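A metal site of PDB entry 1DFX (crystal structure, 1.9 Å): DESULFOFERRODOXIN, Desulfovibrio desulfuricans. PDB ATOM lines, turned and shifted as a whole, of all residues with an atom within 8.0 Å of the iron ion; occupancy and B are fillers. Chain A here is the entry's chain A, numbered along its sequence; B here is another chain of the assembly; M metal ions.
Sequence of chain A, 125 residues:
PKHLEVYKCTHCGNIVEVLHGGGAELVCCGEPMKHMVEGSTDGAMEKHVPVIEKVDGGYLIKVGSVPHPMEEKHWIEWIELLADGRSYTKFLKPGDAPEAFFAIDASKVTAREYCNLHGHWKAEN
The iron ion is bound by SG of Cys 12 (2.3 Å), SG of Cys 9 (2.3 Å), SG of Cys 28 (2.3 Å) and SG of Cys 29 (2.3 Å). The iron ion has four donor atoms within binding distance.
The backbone NH (N) of Ala 24 of chain B lies close to the side-chain sulfur (SG) of Cys 12. The side-chain sulfur of Cys 12 lies close to the side-chain amide oxygen of Asn 14, 3.6 Å away. The backbone NH (N) of Cys 9 lies within hydrogen-bond range of the backbone carbonyl oxygen (O) of Asn 14 (2.8 Å). The side-chain sulfur (SG) of Cys 9 sits close to the backbone NH (N) of His 11. The side-chain amide oxygen (OD1) of Asn 14 sits close to the side-chain sulfur (SG) of Cys 28, 3.5 Å away.
Four residues have an atom within 4 Å of the iron ion: Cys 9, Cys 12, Cys 28 and Cys 29. The nearest printed residue that does not touch the iron ion is Ala 24 of chain B (4.1 Å).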
ATOM      1  N   LYS A   8      24.166  17.100  -1.287  1.00  0.00           N
ATOM      2  CA  LYS A   8      23.504  16.462  -0.138  1.00  0.00           C
ATOM      3  C   LYS A   8      24.481  16.216   0.995  1.00  0.00           C
ATOM      4  O   LYS A   8      25.628  15.844   0.815  1.00  0.00           O
ATOM      5  CB  LYS A   8      22.848  15.144  -0.557  1.00  0.00           C
ATOM      6  CG  LYS A   8      22.580  14.241   0.668  1.00  0.00           C
ATOM      7  CD  LYS A   8      21.914  12.947   0.189  1.00  0.00           C
ATOM      8  CE  LYS A   8      21.626  12.026   1.384  1.00  0.00           C
ATOM      9  NZ  LYS A   8      21.162  10.685   0.894  1.00  0.00           N
ATOM     10  N   CYS A   9      23.977  16.392   2.230  1.00  0.00           N
ATOM     11  CA  CYS A   9      24.873  16.005   3.348  1.00  0.00           C
ATOM     12  C   CYS A   9      24.573  14.505   3.610  1.00  0.00           C
ATOM     13  O   CYS A   9      23.434  14.167   3.906  1.00  0.00           O
ATOM     14  CB  CYS A   9      24.493  16.799   4.603  1.00  0.00           C
ATOM     15  SG  CYS A   9      25.545  16.294   6.023  1.00  0.00           S
ATOM     16  N   THR A  10      25.582  13.669   3.464  1.00  0.00           N
ATOM     17  CA  THR A  10      25.363  12.226   3.685  1.00  0.00           C
ATOM     18  C   THR A  10      25.075  11.916   5.128  1.00  0.00           C
ATOM     19  O   THR A  10      24.362  10.952   5.462  1.00  0.00           O
ATOM     20  CB  THR A  10      26.528  11.393   3.150  1.00  0.00           C
ATOM     21  OG1 THR A  10      27.748  11.796   3.785  1.00  0.00           O
ATOM     22  CG2 THR A  10      26.728  11.652   1.659  1.00  0.00           C
ATOM     23  N   HIS A  11      25.522  12.765   6.059  1.00  0.00           N
ATOM     24  CA  HIS A  11      25.262  12.507   7.463  1.00  0.00           C
ATOM     25  C   HIS A  11      23.889  12.740   7.944  1.00  0.00           C
ATOM     26  O   HIS A  11      23.281  11.889   8.618  1.00  0.00           O
ATOM     27  CB  HIS A  11      26.324  13.219   8.333  1.00  0.00           C
ATOM     28  CG  HIS A  11      27.690  12.663   8.003  1.00  0.00           C
ATOM     29  ND1 HIS A  11      28.570  13.303   7.162  1.00  0.00           N
ATOM     30  CD2 HIS A  11      28.242  11.461   8.292  1.00  0.00           C
ATOM     31  CE1 HIS A  11      29.652  12.551   7.015  1.00  0.00           C
ATOM     32  NE2 HIS A  11      29.480  11.432   7.691  1.00  0.00           N
ATOM     33  N   CYS A  12      23.315  13.930   7.702  1.00  0.00           N
ATOM     34  CA  CYS A  12      22.025  14.295   8.232  1.00  0.00           C
ATOM     35  C   CYS A  12      20.915  14.372   7.208  1.00  0.00           C
ATOM     36  O   CYS A  12      19.751  14.565   7.582  1.00  0.00           O
ATOM     37  CB  CYS A  12      22.122  15.657   8.952  1.00  0.00           C
ATOM     38  SG  CYS A  12      22.398  17.033   7.805  1.00  0.00           S
ATOM     39  N   GLY A  13      21.229  14.285   5.910  1.00  0.00           N
ATOM     40  CA  GLY A  13      20.212  14.261   4.895  1.00  0.00           C
ATOM     41  C   GLY A  13      19.807  15.565   4.294  1.00  0.00           C
ATOM     42  O   GLY A  13      18.911  15.594   3.412  1.00  0.00           O
ATOM     43  N   ASN A  14      20.363  16.686   4.735  1.00  0.00           N
ATOM     44  CA  ASN A  14      19.974  17.984   4.117  1.00  0.00           C
ATOM     45  C   ASN A  14      20.346  17.892   2.613  1.00  0.00           C
ATOM     46  O   ASN A  14      21.385  17.341   2.271  1.00  0.00           O
ATOM     47  CB  ASN A  14      20.886  19.082   4.733  1.00  0.00           C
ATOM     48  CG  ASN A  14      20.383  19.659   6.025  1.00  0.00           C
ATOM     49  OD1 ASN A  14      21.185  20.254   6.797  1.00  0.00           O
ATOM     50  ND2 ASN A  14      19.102  19.596   6.320  1.00  0.00           N
ATOM     51  N   ILE A  15      19.488  18.441   1.784  1.00  0.00           N
ATOM     52  CA  ILE A  15      19.743  18.515   0.343  1.00  0.00           C
ATOM     53  C   ILE A  15      19.364  19.904  -0.146  1.00  0.00           C
ATOM     54  O   ILE A  15      18.308  20.424   0.167  1.00  0.00           O
ATOM     55  CB  ILE A  15      18.936  17.466  -0.447  1.00  0.00           C
ATOM     56  CG1 ILE A  15      19.185  16.032   0.102  1.00  0.00           C
ATOM     57  CG2 ILE A  15      19.431  17.483  -1.925  1.00  0.00           C
ATOM     58  CD1 ILE A  15      18.291  15.017  -0.578  1.00  0.00           C
ATOM     59  N   VAL A  27      29.271  23.308   3.390  1.00  0.00           N
ATOM     60  CA  VAL A  27      29.601  22.322   4.424  1.00  0.00           C
ATOM     61  C   VAL A  27      28.429  22.010   5.317  1.00  0.00           C
ATOM     62  O   VAL A  27      27.573  22.854   5.595  1.00  0.00           O
ATOM     63  CB  VAL A  27      30.781  22.850   5.292  1.00  0.00           C
ATOM     64  CG1 VAL A  27      30.913  22.005   6.535  1.00  0.00           C
ATOM     65  CG2 VAL A  27      32.046  22.855   4.453  1.00  0.00           C
ATOM     66  N   CYS A  28      28.406  20.753   5.782  1.00  0.00           N
ATOM     67  CA  CYS A  28      27.317  20.370   6.704  1.00  0.00           C
ATOM     68  C   CYS A  28      27.803  19.163   7.546  1.00  0.00           C
ATOM     69  O   CYS A  28      28.485  18.311   6.998  1.00  0.00           O
ATOM     70  CB  CYS A  28      26.095  19.943   5.883  1.00  0.00           C
ATOM     71  SG  CYS A  28      24.613  19.678   6.905  1.00  0.00           S
ATOM     72  N   CYS A  29      27.511  19.195   8.839  1.00  0.00           N
ATOM     73  CA  CYS A  29      27.974  18.125   9.744  1.00  0.00           C
ATOM     74  C   CYS A  29      29.479  17.923   9.648  1.00  0.00           C
ATOM     75  O   CYS A  29      29.937  16.766   9.639  1.00  0.00           O
ATOM     76  CB  CYS A  29      27.309  16.791   9.287  1.00  0.00           C
ATOM     77  SG  CYS A  29      25.534  16.771   9.648  1.00  0.00           S
ATOM     78  N   GLY A  30      30.217  19.008   9.563  1.00  0.00           N
ATOM     79  CA  GLY A  30      31.625  19.102   9.485  1.00  0.00           C
ATOM     80  C   GLY A  30      32.286  18.602   8.247  1.00  0.00           C
ATOM     81  O   GLY A  30      33.532  18.605   8.132  1.00  0.00           O
ATOM     82  N   GLU A  31      31.514  18.162   7.248  1.00  0.00           N
ATOM     83  CA  GLU A  31      32.195  17.674   6.008  1.00  0.00           C
ATOM     84  C   GLU A  31      31.621  18.436   4.797  1.00  0.00           C
ATOM     85  O   GLU A  31      30.462  18.809   4.824  1.00  0.00           O
ATOM     86  CB  GLU A  31      31.754  16.184   5.833  1.00  0.00           C
ATOM     87  CG  GLU A  31      32.890  15.210   6.087  1.00  0.00           C
ATOM     88  CD  GLU A  31      32.723  13.945   5.259  1.00  0.00           C
ATOM     89  OE1 GLU A  31      32.088  14.020   4.178  1.00  0.00           O
ATOM     90  OE2 GLU A  31      33.230  12.879   5.679  1.00  0.00           O
ATOM     91  N   MET A  33      29.601  19.092   1.609  1.00  0.00           N
ATOM     92  CA  MET A  33      28.417  18.278   1.197  1.00  0.00           C
ATOM     93  C   MET A  33      28.745  17.556  -0.076  1.00  0.00           C
ATOM     94  O   MET A  33      29.681  17.904  -0.805  1.00  0.00           O
ATOM     95  CB  MET A  33      27.234  19.230   0.971  1.00  0.00           C
ATOM     96  CG  MET A  33      26.814  19.913   2.286  1.00  0.00           C
ATOM     97  SD  MET A  33      25.438  21.016   2.059  1.00  0.00           S
ATOM     98  CE  MET A  33      24.077  19.858   1.882  1.00  0.00           C
ATOM     99  N   PRO B   1      17.479  23.247   8.939  1.00  0.00           N
ATOM    100  CA  PRO B   1      16.775  24.039   7.926  1.00  0.00           C
ATOM    101  C   PRO B   1      15.483  23.332   7.477  1.00  0.00           C
ATOM    102  O   PRO B   1      15.379  22.123   7.637  1.00  0.00           O
ATOM    103  CB  PRO B   1      17.764  24.101   6.778  1.00  0.00           C
ATOM    104  CG  PRO B   1      18.767  23.059   6.999  1.00  0.00           C
ATOM    105  CD  PRO B   1      18.526  22.417   8.332  1.00  0.00           C
ATOM    106  N   GLY B  22      15.633  19.389   7.641  1.00  0.00           N
ATOM    107  CA  GLY B  22      15.585  18.630   8.874  1.00  0.00           C
ATOM    108  C   GLY B  22      16.902  18.228   9.453  1.00  0.00           C
ATOM    109  O   GLY B  22      16.959  17.644  10.554  1.00  0.00           O
ATOM    110  N   GLY B  23      18.014  18.519   8.785  1.00  0.00           N
ATOM    111  CA  GLY B  23      19.332  18.168   9.224  1.00  0.00           C
ATOM    112  C   GLY B  23      20.006  19.196  10.092  1.00  0.00           C
ATOM    113  O   GLY B  23      19.363  19.979  10.789  1.00  0.00           O
ATOM    114  N   ALA B  24      21.338  19.179  10.079  1.00  0.00           N
ATOM    115  CA  ALA B  24      22.123  20.122  10.886  1.00  0.00           C
ATOM    116  C   ALA B  24      22.173  21.485  10.175  1.00  0.00           C
ATOM    117  O   ALA B  24      21.640  21.624   9.063  1.00  0.00           O
ATOM    118  CB  ALA B  24      23.550  19.591  11.020  1.00  0.00           C
ATOM    119  N   GLU B  25      22.835  22.436  10.820  1.00  0.00           N
ATOM    120  CA  GLU B  25      22.955  23.779  10.241  1.00  0.00           C
ATOM    121  C   GLU B  25      23.822  23.727   8.988  1.00  0.00           C
ATOM    122  O   GLU B  25      24.871  23.097   8.959  1.00  0.00           O
ATOM    123  CB  GLU B  25      23.645  24.711  11.254  1.00  0.00           C
ATOM    124  CG  GLU B  25      22.775  25.082  12.431  1.00  0.00           C
ATOM    125  CD  GLU B  25      23.464  26.053  13.375  1.00  0.00           C
ATOM    126  OE1 GLU B  25      24.710  25.987  13.461  1.00  0.00           O
ATOM    127  OE2 GLU B  25      22.768  26.877  13.995  1.00  0.00           O
ATOM    128  N   LEU B  26      23.368  24.427   7.932  1.00  0.00           N
ATOM    129  CA  LEU B  26      24.241  24.436   6.727  1.00  0.00           C
ATOM    130  C   LEU B  26      25.401  25.379   7.022  1.00  0.00           C
ATOM    131  O   LEU B  26      25.211  26.437   7.629  1.00  0.00           O
ATOM    132  CB  LEU B  26      23.418  24.964   5.547  1.00  0.00           C
ATOM    133  CG  LEU B  26      22.277  24.020   5.130  1.00  0.00           C
ATOM    134  CD1 LEU B  26      21.298  24.745   4.216  1.00  0.00           C
ATOM    135  CD2 LEU B  26      22.870  22.803   4.430  1.00  0.00           C
ATOM    136  N   VAL B  27      26.593  24.984   6.590  1.00  0.00           N
ATOM    137  CA  VAL B  27      27.753  25.823   6.881  1.00  0.00           C
ATOM    138  C   VAL B  27      28.537  26.173   5.643  1.00  0.00           C
ATOM    139  O   VAL B  27      28.630  25.401   4.683  1.00  0.00           O
ATOM    140  CB  VAL B  27      28.680  25.094   7.899  1.00  0.00           C
ATOM    141  CG1 VAL B  27      30.025  25.786   7.954  1.00  0.00           C
ATOM    142  CG2 VAL B  27      27.989  25.028   9.242  1.00  0.00           C
HETATM  143 FE    FE M   1      24.593  17.525   7.654  1.00  0.00          FE
